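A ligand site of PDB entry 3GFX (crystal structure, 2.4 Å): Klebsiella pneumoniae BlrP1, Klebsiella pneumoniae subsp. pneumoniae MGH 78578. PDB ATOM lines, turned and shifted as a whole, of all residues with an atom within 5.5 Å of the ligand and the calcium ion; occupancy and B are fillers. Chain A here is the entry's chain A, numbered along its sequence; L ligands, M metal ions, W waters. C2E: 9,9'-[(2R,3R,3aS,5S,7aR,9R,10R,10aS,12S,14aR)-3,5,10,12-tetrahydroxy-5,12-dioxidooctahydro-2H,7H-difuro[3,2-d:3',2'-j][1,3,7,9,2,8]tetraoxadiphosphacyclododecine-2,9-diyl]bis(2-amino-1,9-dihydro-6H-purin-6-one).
OE1 of Gln 182 sits at hydrogen-bond distance from NE2 of Gln 387 (2.8 Å).
The backbone carbonyl oxygen (O) of Ser 392 lies within hydrogen-bond range of the side-chain amide nitrogen (NE2) of Gln 182.
The backbone NH (N) of Val 369 is in hydrogen-bond range of the backbone carbonyl oxygen (O) of Gln 387, at 3.1 Å.
The side-chain hydroxyl (OG) of Ser 226 is in hydrogen-bond range of the side-chain amino group (NZ) of Lys 227 (3.1 Å).
N of Glu 196 sits at hydrogen-bond distance from O of Gln 182.
The side-chain carboxylate (OE1) of Glu 196 sits at hydrogen-bond distance from the side-chain amide nitrogen (NE2) of Gln 387.
O of Ala 197 lies within hydrogen-bond range of ND2 of Asn 247, 3.2 Å away.
The backbone NH of Gly 368 is in hydrogen-bond range of the backbone carbonyl oxygen of Gln 387, 3.0 Å away.
An oxygen (O2P) of the ligand binds the calcium ion (2.2 Å).
OD2 of Asp 310 binds the calcium ion, at 2.3 Å.
OE2 of Glu 280 binds the calcium ion, 2.4 Å away.
OE2 of Glu 196 is bound to the calcium ion, at 2.4 Å.
OD1 of Asn 247 binds the calcium ion, at 2.5 Å.
Water W7 binds the calcium ion.
Water W7 lies within hydrogen-bond range of OE1 of Glu 367 (2.6 Å), OE1 of Glu 196 (2.8 Å) and NZ of Lys 331 (2.9 Å).
Water W9 bridges O1P of the ligand (2.7 Å) and OD2 of Asp 311 (3.2 Å).
Water W5 lies within hydrogen-bond range of N of Gly 368, N7 of the ligand and O of Gln 387.
Water W2 lies within hydrogen-bond range of the side-chain carboxylate of Glu 370 and a nitrogen (N2) of the ligand.
Water W4 lies within hydrogen-bond range of the backbone carbonyl oxygen (O) of Ala 197 (2.6 Å), the backbone NH (N) of Asn 247 (2.9 Å) and an oxygen (O61) of the ligand (3.2 Å).
Of the 30 residues printed, 4 come within 4 Å of the calcium ion.
The backbone carbonyl oxygen (O) of Asn 247 lies within hydrogen-bond range of a nitrogen (N11) of the ligand.
OD1 of Asp 223 is in hydrogen-bond range of N11 of the ligand, at 2.9 Å.
NZ of Lys 227 is in hydrogen-bond range of O61 of the ligand.
An oxygen (O11) of the ligand lies within salt-bridge range of the guanidinium group of Arg 200, 2.8 Å away.
N of Ile 199 is in hydrogen-bond range of N71 of the ligand.
NE2 of Gln 182 sits at hydrogen-bond distance from N7 of the ligand, at 3.1 Å.
O6 of the ligand is in hydrogen-bond range of N of Phe 389, at 2.8 Å.
OE1 of Glu 370 is in hydrogen-bond range of N1 of the ligand (2.9 Å).
Residues that only touch the ligand: Gly 388, Pro 207, Leu 198, Pro 394, Gly 368, Asp 311, Val 369, Phe 211, Phe 179 and Leu 249.
Within 4 Å of the ligand: Phe 179, Gln 182, Glu 196, Leu 198, Ile 199, Arg 200, Pro 207, Phe 211, Asp 223, Lys 227, Asn 247, Leu 249, Asp 310, Asp 311, Gly 368, Val 369, Glu 370, Gly 388, Phe 389 and Pro 394.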
ATOM      1  N   PHE A 179      -0.735  -3.264  29.295  1.00  0.00           N
ATOM      2  CA  PHE A 179      -1.238  -3.114  27.935  1.00  0.00           C
ATOM      3  C   PHE A 179      -0.100  -2.946  26.930  1.00  0.00           C
ATOM      4  O   PHE A 179       0.813  -2.147  27.139  1.00  0.00           O
ATOM      5  CB  PHE A 179      -2.208  -1.939  27.828  1.00  0.00           C
ATOM      6  CG  PHE A 179      -3.591  -2.251  28.338  1.00  0.00           C
ATOM      7  CD1 PHE A 179      -3.916  -2.032  29.665  1.00  0.00           C
ATOM      8  CD2 PHE A 179      -4.551  -2.765  27.484  1.00  0.00           C
ATOM      9  CE1 PHE A 179      -5.185  -2.324  30.135  1.00  0.00           C
ATOM     10  CE2 PHE A 179      -5.833  -3.058  27.949  1.00  0.00           C
ATOM     11  CZ  PHE A 179      -6.136  -2.828  29.276  1.00  0.00           C
ATOM     12  N   GLN A 182      -0.142  -1.299  19.747  1.00  0.00           N
ATOM     13  CA  GLN A 182       0.154  -1.474  18.332  1.00  0.00           C
ATOM     14  C   GLN A 182      -0.438  -0.330  17.521  1.00  0.00           C
ATOM     15  O   GLN A 182      -1.609   0.023  17.686  1.00  0.00           O
ATOM     16  CB  GLN A 182      -0.369  -2.818  17.812  1.00  0.00           C
ATOM     17  CG  GLN A 182       0.164  -3.191  16.432  1.00  0.00           C
ATOM     18  CD  GLN A 182      -0.416  -4.482  15.893  1.00  0.00           C
ATOM     19  OE1 GLN A 182      -1.502  -4.898  16.287  1.00  0.00           O
ATOM     20  NE2 GLN A 182       0.308  -5.108  14.978  1.00  0.00           N
ATOM     21  N   GLU A 196      -3.787   0.844  19.256  1.00  0.00           N
ATOM     22  CA  GLU A 196      -4.707  -0.101  19.887  1.00  0.00           C
ATOM     23  C   GLU A 196      -4.094  -0.701  21.143  1.00  0.00           C
ATOM     24  O   GLU A 196      -2.966  -1.190  21.134  1.00  0.00           O
ATOM     25  CB  GLU A 196      -5.113  -1.213  18.912  1.00  0.00           C
ATOM     26  CG  GLU A 196      -6.234  -2.099  19.461  1.00  0.00           C
ATOM     27  CD  GLU A 196      -6.445  -3.370  18.658  1.00  0.00           C
ATOM     28  OE1 GLU A 196      -5.772  -3.562  17.623  1.00  0.00           O
ATOM     29  OE2 GLU A 196      -7.308  -4.178  19.061  1.00  0.00           O
ATOM     30  N   ALA A 197      -4.862  -0.662  22.233  1.00  0.00           N
ATOM     31  CA  ALA A 197      -4.434  -1.215  23.510  1.00  0.00           C
ATOM     32  C   ALA A 197      -4.785  -2.698  23.622  1.00  0.00           C
ATOM     33  O   ALA A 197      -5.960  -3.081  23.561  1.00  0.00           O
ATOM     34  CB  ALA A 197      -5.064  -0.434  24.657  1.00  0.00           C
ATOM     35  N   LEU A 198      -3.758  -3.533  23.755  1.00  0.00           N
ATOM     36  CA  LEU A 198      -3.922  -4.970  23.851  1.00  0.00           C
ATOM     37  C   LEU A 198      -3.470  -5.445  25.224  1.00  0.00           C
ATOM     38  O   LEU A 198      -2.310  -5.278  25.594  1.00  0.00           O
ATOM     39  CB  LEU A 198      -3.107  -5.676  22.760  1.00  0.00           C
ATOM     40  CG  LEU A 198      -3.428  -5.275  21.317  1.00  0.00           C
ATOM     41  CD1 LEU A 198      -2.274  -5.625  20.385  1.00  0.00           C
ATOM     42  CD2 LEU A 198      -4.731  -5.900  20.833  1.00  0.00           C
ATOM     43  N   ILE A 199      -4.383  -6.044  25.985  1.00  0.00           N
ATOM     44  CA  ILE A 199      -4.134  -6.381  27.386  1.00  0.00           C
ATOM     45  C   ILE A 199      -3.068  -7.475  27.563  1.00  0.00           C
ATOM     46  O   ILE A 199      -2.943  -8.381  26.732  1.00  0.00           O
ATOM     47  CB  ILE A 199      -5.462  -6.743  28.134  1.00  0.00           C
ATOM     48  CG1 ILE A 199      -5.314  -6.520  29.651  1.00  0.00           C
ATOM     49  CG2 ILE A 199      -5.950  -8.153  27.807  1.00  0.00           C
ATOM     50  CD1 ILE A 199      -6.616  -6.611  30.418  1.00  0.00           C
ATOM     51  N   ARG A 200      -2.299  -7.346  28.603  1.00  0.00           N
ATOM     52  CA  ARG A 200      -1.294  -8.326  28.954  1.00  0.00           C
ATOM     53  C   ARG A 200      -1.400  -8.634  30.439  1.00  0.00           C
ATOM     54  O   ARG A 200      -1.898  -7.809  31.206  1.00  0.00           O
ATOM     55  CB  ARG A 200       0.116  -7.812  28.608  1.00  0.00           C
ATOM     56  CG  ARG A 200       0.355  -7.486  27.134  1.00  0.00           C
ATOM     57  CD  ARG A 200       0.557  -8.738  26.303  1.00  0.00           C
ATOM     58  NE  ARG A 200       0.789  -8.455  24.891  1.00  0.00           N
ATOM     59  CZ  ARG A 200      -0.150  -8.506  23.941  1.00  0.00           C
ATOM     60  NH1 ARG A 200      -1.393  -8.841  24.254  1.00  0.00           N
ATOM     61  NH2 ARG A 200       0.166  -8.222  22.682  1.00  0.00           N
ATOM     62  N   SER A 206      -0.420 -13.391  27.318  1.00  0.00           N
ATOM     63  CA  SER A 206      -1.474 -13.047  26.355  1.00  0.00           C
ATOM     64  C   SER A 206      -2.780 -12.623  27.041  1.00  0.00           C
ATOM     65  O   SER A 206      -2.943 -12.828  28.246  1.00  0.00           O
ATOM     66  CB  SER A 206      -1.706 -14.254  25.441  1.00  0.00           C
ATOM     67  OG  SER A 206      -2.188 -15.364  26.168  1.00  0.00           O
ATOM     68  N   PRO A 207      -3.716 -12.010  26.274  1.00  0.00           N
ATOM     69  CA  PRO A 207      -5.081 -11.752  26.770  1.00  0.00           C
ATOM     70  C   PRO A 207      -5.803 -13.000  27.282  1.00  0.00           C
ATOM     71  O   PRO A 207      -6.582 -12.906  28.217  1.00  0.00           O
ATOM     72  CB  PRO A 207      -5.791 -11.186  25.535  1.00  0.00           C
ATOM     73  CG  PRO A 207      -4.707 -10.557  24.758  1.00  0.00           C
ATOM     74  CD  PRO A 207      -3.544 -11.476  24.908  1.00  0.00           C
ATOM     75  N   PHE A 211      -7.172 -13.282  31.190  1.00  0.00           N
ATOM     76  CA  PHE A 211      -8.582 -13.543  31.549  1.00  0.00           C
ATOM     77  C   PHE A 211      -8.809 -14.907  32.215  1.00  0.00           C
ATOM     78  O   PHE A 211      -9.780 -15.079  32.950  1.00  0.00           O
ATOM     79  CB  PHE A 211      -9.503 -13.366  30.338  1.00  0.00           C
ATOM     80  CG  PHE A 211      -9.846 -11.929  30.041  1.00  0.00           C
ATOM     81  CD1 PHE A 211     -10.849 -11.279  30.748  1.00  0.00           C
ATOM     82  CD2 PHE A 211      -9.162 -11.220  29.048  1.00  0.00           C
ATOM     83  CE1 PHE A 211     -11.169  -9.953  30.474  1.00  0.00           C
ATOM     84  CE2 PHE A 211      -9.475  -9.899  28.775  1.00  0.00           C
ATOM     85  CZ  PHE A 211     -10.479  -9.266  29.487  1.00  0.00           C
ATOM     86  N   ASP A 223     -12.704  -6.617  32.589  1.00  0.00           N
ATOM     87  CA  ASP A 223     -12.512  -6.074  31.233  1.00  0.00           C
ATOM     88  C   ASP A 223     -12.777  -4.577  31.192  1.00  0.00           C
ATOM     89  O   ASP A 223     -12.032  -3.823  30.576  1.00  0.00           O
ATOM     90  CB  ASP A 223     -13.420  -6.816  30.249  1.00  0.00           C
ATOM     91  CG  ASP A 223     -13.083  -6.524  28.801  1.00  0.00           C
ATOM     92  OD1 ASP A 223     -11.996  -5.992  28.516  1.00  0.00           O
ATOM     93  OD2 ASP A 223     -13.921  -6.831  27.928  1.00  0.00           O
ATOM     94  N   SER A 226     -10.105  -2.693  33.813  1.00  0.00           N
ATOM     95  CA  SER A 226      -8.721  -2.722  33.321  1.00  0.00           C
ATOM     96  C   SER A 226      -8.392  -1.545  32.411  1.00  0.00           C
ATOM     97  O   SER A 226      -7.230  -1.169  32.255  1.00  0.00           O
ATOM     98  CB  SER A 226      -8.440  -4.024  32.572  1.00  0.00           C
ATOM     99  OG  SER A 226      -9.246  -4.140  31.411  1.00  0.00           O
ATOM    100  N   LYS A 227      -9.430  -0.959  31.829  1.00  0.00           N
ATOM    101  CA  LYS A 227      -9.287   0.125  30.846  1.00  0.00           C
ATOM    102  C   LYS A 227      -8.740   1.416  31.428  1.00  0.00           C
ATOM    103  O   LYS A 227      -8.221   2.255  30.695  1.00  0.00           O
ATOM    104  CB  LYS A 227     -10.620   0.384  30.142  1.00  0.00           C
ATOM    105  CG  LYS A 227     -11.123  -0.800  29.331  1.00  0.00           C
ATOM    106  CD  LYS A 227     -10.064  -1.273  28.353  1.00  0.00           C
ATOM    107  CE  LYS A 227     -10.460  -2.556  27.675  1.00  0.00           C
ATOM    108  NZ  LYS A 227     -10.320  -3.745  28.537  1.00  0.00           N
ATOM    109  N   ASN A 247     -10.282  -2.595  23.442  1.00  0.00           N
ATOM    110  CA  ASN A 247     -11.114  -3.773  23.215  1.00  0.00           C
ATOM    111  C   ASN A 247     -12.024  -4.060  24.394  1.00  0.00           C
ATOM    112  O   ASN A 247     -11.564  -4.239  25.521  1.00  0.00           O
ATOM    113  CB  ASN A 247     -10.239  -5.000  22.953  1.00  0.00           C
ATOM    114  CG  ASN A 247      -9.458  -4.885  21.667  1.00  0.00           C
ATOM    115  OD1 ASN A 247     -10.007  -5.103  20.586  1.00  0.00           O
ATOM    116  ND2 ASN A 247      -8.178  -4.560  21.762  1.00  0.00           N
ATOM    117  N   LEU A 248     -13.330  -4.133  24.127  1.00  0.00           N
ATOM    118  CA  LEU A 248     -14.300  -4.452  25.176  1.00  0.00           C
ATOM    119  C   LEU A 248     -15.316  -5.472  24.691  1.00  0.00           C
ATOM    120  O   LEU A 248     -15.734  -5.453  23.526  1.00  0.00           O
ATOM    121  CB  LEU A 248     -15.021  -3.191  25.660  1.00  0.00           C
ATOM    122  CG  LEU A 248     -14.312  -2.304  26.676  1.00  0.00           C
ATOM    123  CD1 LEU A 248     -15.007  -0.951  26.787  1.00  0.00           C
ATOM    124  CD2 LEU A 248     -14.241  -2.985  28.048  1.00  0.00           C
ATOM    125  N   LEU A 249     -15.704  -6.377  25.588  1.00  0.00           N
ATOM    126  CA  LEU A 249     -16.863  -7.240  25.358  1.00  0.00           C
ATOM    127  C   LEU A 249     -18.108  -6.370  25.482  1.00  0.00           C
ATOM    128  O   LEU A 249     -18.171  -5.508  26.357  1.00  0.00           O
ATOM    129  CB  LEU A 249     -16.896  -8.373  26.379  1.00  0.00           C
ATOM    130  CG  LEU A 249     -15.841  -9.485  26.260  1.00  0.00           C
ATOM    131  CD1 LEU A 249     -15.664 -10.205  27.584  1.00  0.00           C
ATOM    132  CD2 LEU A 249     -16.196 -10.465  25.153  1.00  0.00           C
ATOM    133  N   GLU A 280     -13.739  -0.931  20.630  1.00  0.00           N
ATOM    134  CA  GLU A 280     -13.742  -2.039  19.696  1.00  0.00           C
ATOM    135  C   GLU A 280     -14.558  -3.227  20.200  1.00  0.00           C
ATOM    136  O   GLU A 280     -14.211  -3.844  21.208  1.00  0.00           O
ATOM    137  CB  GLU A 280     -12.325  -2.475  19.347  1.00  0.00           C
ATOM    138  CG  GLU A 280     -11.676  -1.654  18.249  1.00  0.00           C
ATOM    139  CD  GLU A 280     -10.304  -2.164  17.874  1.00  0.00           C
ATOM    140  OE1 GLU A 280      -9.434  -1.333  17.568  1.00  0.00           O
ATOM    141  OE2 GLU A 280     -10.091  -3.402  17.867  1.00  0.00           O
ATOM    142  N   ASP A 310     -14.825  -4.698  15.131  1.00  0.00           N
ATOM    143  CA  ASP A 310     -13.610  -5.464  14.913  1.00  0.00           C
ATOM    144  C   ASP A 310     -13.924  -6.825  14.312  1.00  0.00           C
ATOM    145  O   ASP A 310     -15.040  -7.333  14.471  1.00  0.00           O
ATOM    146  CB  ASP A 310     -12.847  -5.608  16.229  1.00  0.00           C
ATOM    147  CG  ASP A 310     -11.397  -5.980  16.020  1.00  0.00           C
ATOM    148  OD1 ASP A 310     -10.851  -5.723  14.917  1.00  0.00           O
ATOM    149  OD2 ASP A 310     -10.779  -6.519  16.963  1.00  0.00           O
ATOM    150  N   ASP A 311     -12.936  -7.409  13.629  1.00  0.00           N
ATOM    151  CA  ASP A 311     -13.071  -8.698  12.927  1.00  0.00           C
ATOM    152  C   ASP A 311     -14.264  -8.722  11.977  1.00  0.00           C
ATOM    153  O   ASP A 311     -15.019  -9.699  11.922  1.00  0.00           O
ATOM    154  CB  ASP A 311     -13.145  -9.868  13.923  1.00  0.00           C
ATOM    155  CG  ASP A 311     -11.882 -10.014  14.764  1.00  0.00           C
ATOM    156  OD1 ASP A 311     -10.779  -9.807  14.231  1.00  0.00           O
ATOM    157  OD2 ASP A 311     -12.009 -10.350  15.958  1.00  0.00           O
ATOM    158  N   LYS A 331     -12.942  -2.820  11.082  1.00  0.00           N
ATOM    159  CA  LYS A 331     -11.631  -3.413  10.914  1.00  0.00           C
ATOM    160  C   LYS A 331     -11.776  -4.774  10.233  1.00  0.00           C
ATOM    161  O   LYS A 331     -12.269  -5.730  10.844  1.00  0.00           O
ATOM    162  CB  LYS A 331     -10.911  -3.541  12.262  1.00  0.00           C
ATOM    163  CG  LYS A 331     -10.931  -2.244  13.085  1.00  0.00           C
ATOM    164  CD  LYS A 331     -10.212  -2.409  14.401  1.00  0.00           C
ATOM    165  CE  LYS A 331      -8.783  -1.920  14.321  1.00  0.00           C
ATOM    166  NZ  LYS A 331      -7.971  -2.413  15.460  1.00  0.00           N
ATOM    167  N   GLU A 367      -6.661  -5.601   8.979  1.00  0.00           N
ATOM    168  CA  GLU A 367      -6.008  -6.289  10.093  1.00  0.00           C
ATOM    169  C   GLU A 367      -5.024  -7.344   9.621  1.00  0.00           C
ATOM    170  O   GLU A 367      -5.202  -7.931   8.555  1.00  0.00           O
ATOM    171  CB  GLU A 367      -7.056  -6.985  10.965  1.00  0.00           C
ATOM    172  CG  GLU A 367      -8.046  -6.072  11.649  1.00  0.00           C
ATOM    173  CD  GLU A 367      -7.517  -5.556  12.959  1.00  0.00           C
ATOM    174  OE1 GLU A 367      -7.358  -6.363  13.900  1.00  0.00           O
ATOM    175  OE2 GLU A 367      -7.253  -4.346  13.038  1.00  0.00           O
ATOM    176  N   GLY A 368      -4.009  -7.603  10.437  1.00  0.00           N
ATOM    177  CA  GLY A 368      -3.082  -8.713  10.216  1.00  0.00           C
ATOM    178  C   GLY A 368      -2.287  -8.646   8.922  1.00  0.00           C
ATOM    179  O   GLY A 368      -2.033  -9.662   8.286  1.00  0.00           O
ATOM    180  N   VAL A 369      -1.896  -7.428   8.543  1.00  0.00           N
ATOM    181  CA  VAL A 369      -1.114  -7.205   7.331  1.00  0.00           C
ATOM    182  C   VAL A 369       0.343  -7.582   7.586  1.00  0.00           C
ATOM    183  O   VAL A 369       1.056  -6.886   8.298  1.00  0.00           O
ATOM    184  CB  VAL A 369      -1.227  -5.744   6.852  1.00  0.00           C
ATOM    185  CG1 VAL A 369      -0.664  -5.599   5.438  1.00  0.00           C
ATOM    186  CG2 VAL A 369      -2.669  -5.263   6.907  1.00  0.00           C
ATOM    187  N   GLU A 370       0.764  -8.701   7.007  1.00  0.00           N
ATOM    188  CA  GLU A 370       2.075  -9.281   7.284  1.00  0.00           C
ATOM    189  C   GLU A 370       3.093  -9.106   6.159  1.00  0.00           C
ATOM    190  O   GLU A 370       4.305  -9.102   6.405  1.00  0.00           O
ATOM    191  CB  GLU A 370       1.941 -10.765   7.620  1.00  0.00           C
ATOM    192  CG  GLU A 370       1.161 -11.068   8.899  1.00  0.00           C
ATOM    193  CD  GLU A 370       1.121 -12.550   9.227  1.00  0.00           C
ATOM    194  OE1 GLU A 370       1.050 -12.898  10.417  1.00  0.00           O
ATOM    195  OE2 GLU A 370       1.169 -13.379   8.290  1.00  0.00           O
ATOM    196  N   GLN A 387      -2.995  -2.222   9.835  1.00  0.00           N
ATOM    197  CA  GLN A 387      -2.500  -2.727  11.106  1.00  0.00           C
ATOM    198  C   GLN A 387      -1.925  -4.130  10.904  1.00  0.00           C
ATOM    199  O   GLN A 387      -2.600  -5.002  10.356  1.00  0.00           O
ATOM    200  CB  GLN A 387      -3.610  -2.759  12.148  1.00  0.00           C
ATOM    201  CG  GLN A 387      -3.126  -3.047  13.562  1.00  0.00           C
ATOM    202  CD  GLN A 387      -4.249  -3.134  14.573  1.00  0.00           C
ATOM    203  OE1 GLN A 387      -5.358  -2.634  14.339  1.00  0.00           O
ATOM    204  NE2 GLN A 387      -3.989  -3.770  15.709  1.00  0.00           N
ATOM    205  N   GLY A 388      -0.692  -4.330  11.366  1.00  0.00           N
ATOM    206  CA  GLY A 388      -0.047  -5.625  11.219  1.00  0.00           C
ATOM    207  C   GLY A 388       1.442  -5.611  11.516  1.00  0.00           C
ATOM    208  O   GLY A 388       2.041  -4.539  11.660  1.00  0.00           O
ATOM    209  N   PHE A 389       2.038  -6.800  11.590  1.00  0.00           N
ATOM    210  CA  PHE A 389       3.441  -6.973  11.947  1.00  0.00           C
ATOM    211  C   PHE A 389       4.423  -6.400  10.917  1.00  0.00           C
ATOM    212  O   PHE A 389       5.591  -6.184  11.238  1.00  0.00           O
ATOM    213  CB  PHE A 389       3.761  -8.465  12.175  1.00  0.00           C
ATOM    214  CG  PHE A 389       3.145  -9.049  13.416  1.00  0.00           C
ATOM    215  CD1 PHE A 389       2.727  -8.251  14.471  1.00  0.00           C
ATOM    216  CD2 PHE A 389       3.003 -10.438  13.544  1.00  0.00           C
ATOM    217  CE1 PHE A 389       2.154  -8.800  15.616  1.00  0.00           C
ATOM    218  CE2 PHE A 389       2.449 -10.997  14.683  1.00  0.00           C
ATOM    219  CZ  PHE A 389       2.022 -10.182  15.716  1.00  0.00           C
ATOM    220  N   LEU A 390       3.929  -6.150   9.709  1.00  0.00           N
ATOM    221  CA  LEU A 390       4.733  -5.545   8.644  1.00  0.00           C
ATOM    222  C   LEU A 390       5.159  -4.123   9.007  1.00  0.00           C
ATOM    223  O   LEU A 390       6.285  -3.707   8.705  1.00  0.00           O
ATOM    224  CB  LEU A 390       3.949  -5.537   7.327  1.00  0.00           C
ATOM    225  CG  LEU A 390       4.661  -5.078   6.055  1.00  0.00           C
ATOM    226  CD1 LEU A 390       5.677  -6.112   5.578  1.00  0.00           C
ATOM    227  CD2 LEU A 390       3.649  -4.771   4.955  1.00  0.00           C
ATOM    228  N   SER A 392       4.147  -2.394  12.366  1.00  0.00           N
ATOM    229  CA  SER A 392       4.357  -2.193  13.789  1.00  0.00           C
ATOM    230  C   SER A 392       3.937  -3.416  14.608  1.00  0.00           C
ATOM    231  O   SER A 392       2.833  -3.935  14.449  1.00  0.00           O
ATOM    232  CB  SER A 392       3.585  -0.961  14.268  1.00  0.00           C
ATOM    233  OG  SER A 392       3.738  -0.755  15.661  1.00  0.00           O
ATOM    234  N   PRO A 394       3.227  -5.033  18.497  1.00  0.00           N
ATOM    235  CA  PRO A 394       2.770  -4.552  19.802  1.00  0.00           C
ATOM    236  C   PRO A 394       3.916  -4.328  20.778  1.00  0.00           C
ATOM    237  O   PRO A 394       4.810  -5.170  20.883  1.00  0.00           O
ATOM    238  CB  PRO A 394       1.856  -5.686  20.295  1.00  0.00           C
ATOM    239  CG  PRO A 394       1.415  -6.383  19.068  1.00  0.00           C
ATOM    240  CD  PRO A 394       2.591  -6.313  18.138  1.00  0.00           C
HETATM  241  P1  C2E L   1      -7.628  -8.477  18.037  1.00  0.00           P
HETATM  242  O2P C2E L   1      -7.800  -7.147  18.735  1.00  0.00           O
HETATM  243  O1P C2E L   1      -8.689  -8.914  17.057  1.00  0.00           O
HETATM  244  O5' C2E L   1      -6.253  -8.435  17.208  1.00  0.00           O
HETATM  245  C5' C2E L   1      -5.009  -8.082  17.793  1.00  0.00           C
HETATM  246  C4' C2E L   1      -4.150  -9.335  17.947  1.00  0.00           C
HETATM  247  O4' C2E L   1      -3.648  -9.742  16.668  1.00  0.00           O
HETATM  248  C3' C2E L   1      -2.941  -9.055  18.808  1.00  0.00           C
HETATM  249  O3' C2E L   1      -2.673 -10.177  19.626  1.00  0.00           O
HETATM  250  C2' C2E L   1      -1.836  -8.940  17.820  1.00  0.00           C
HETATM  251  O2' C2E L   1      -0.568  -9.014  18.231  1.00  0.00           O
HETATM  252  C1' C2E L   1      -2.215  -9.457  16.654  1.00  0.00           C
HETATM  253  N9  C2E L   1      -1.657  -9.056  15.474  1.00  0.00           N
HETATM  254  C8  C2E L   1      -1.489  -7.827  15.157  1.00  0.00           C
HETATM  255  N7  C2E L   1      -0.948  -7.791  13.991  1.00  0.00           N
HETATM  256  C5  C2E L   1      -0.764  -9.050  13.517  1.00  0.00           C
HETATM  257  C6  C2E L   1      -0.241  -9.602  12.348  1.00  0.00           C
HETATM  258  O6  C2E L   1       0.192  -8.882  11.429  1.00  0.00           O
HETATM  259  N1  C2E L   1      -0.217 -10.946  12.220  1.00  0.00           N
HETATM  260  C2  C2E L   1      -0.678 -11.750  13.205  1.00  0.00           C
HETATM  261  N2  C2E L   1      -0.632 -13.093  13.019  1.00  0.00           N
HETATM  262  N3  C2E L   1      -1.191 -11.237  14.355  1.00  0.00           N
HETATM  263  C4  C2E L   1      -1.236  -9.897  14.519  1.00  0.00           C
HETATM  264  P11 C2E L   1      -3.228 -10.282  21.131  1.00  0.00           P
HETATM  265  O21 C2E L   1      -2.321 -11.412  21.834  1.00  0.00           O
HETATM  266  O11 C2E L   1      -2.858  -8.919  21.898  1.00  0.00           O
HETATM  267  O5A C2E L   1      -4.836 -10.282  21.190  1.00  0.00           O
HETATM  268  C5A C2E L   1      -5.631 -11.459  21.253  1.00  0.00           C
HETATM  269  C4A C2E L   1      -7.010 -10.788  21.251  1.00  0.00           C
HETATM  270  O4A C2E L   1      -7.409 -10.466  22.590  1.00  0.00           O
HETATM  271  C3A C2E L   1      -7.096  -9.470  20.478  1.00  0.00           C
HETATM  272  O3A C2E L   1      -7.451  -9.663  19.112  1.00  0.00           O
HETATM  273  C2A C2E L   1      -8.115  -8.686  21.260  1.00  0.00           C
HETATM  274  O2A C2E L   1      -9.342  -9.126  20.955  1.00  0.00           O
HETATM  275  C1A C2E L   1      -7.810  -9.080  22.490  1.00  0.00           C
HETATM  276  N91 C2E L   1      -7.765  -8.200  23.531  1.00  0.00           N
HETATM  277  C81 C2E L   1      -6.665  -7.486  23.764  1.00  0.00           C
HETATM  278  N71 C2E L   1      -6.978  -6.730  24.847  1.00  0.00           N
HETATM  279  C51 C2E L   1      -8.246  -7.004  25.233  1.00  0.00           C
HETATM  280  C61 C2E L   1      -9.059  -6.526  26.262  1.00  0.00           C
HETATM  281  O61 C2E L   1      -8.622  -5.662  27.049  1.00  0.00           O
HETATM  282  N11 C2E L   1     -10.308  -7.011  26.388  1.00  0.00           N
HETATM  283  C21 C2E L   1     -10.792  -7.943  25.543  1.00  0.00           C
HETATM  284  N21 C2E L   1     -12.067  -8.405  25.710  1.00  0.00           N
HETATM  285  N31 C2E L   1     -10.030  -8.431  24.526  1.00  0.00           N
HETATM  286  C41 C2E L   1      -8.769  -7.968  24.376  1.00  0.00           C
HETATM  287 CA    CA M   1      -9.160  -5.521  18.319  1.00  0.00          CA
HETATM  288  O   HOH W   1      -4.301 -10.037  13.431  1.00  0.00           O
HETATM  289  O   HOH W   2       0.072 -15.444  11.094  1.00  0.00           O
HETATM  290  O   HOH W   3      -0.328 -12.369  22.825  1.00  0.00           O
HETATM  291  O   HOH W   4      -8.056  -3.250  25.100  1.00  0.00           O
HETATM  292  O   HOH W   5      -3.594  -6.856  13.036  1.00  0.00           O
HETATM  293  O   HOH W   6       0.178 -11.271  19.159  1.00  0.00           O
HETATM  294  O   HOH W   7      -7.555  -5.183  16.256  1.00  0.00           O
HETATM  295  O   HOH W   8      -3.434 -12.566  11.705  1.00  0.00           O
HETATM  296  O   HOH W   9     -10.881  -8.977  18.610  1.00  0.00           O
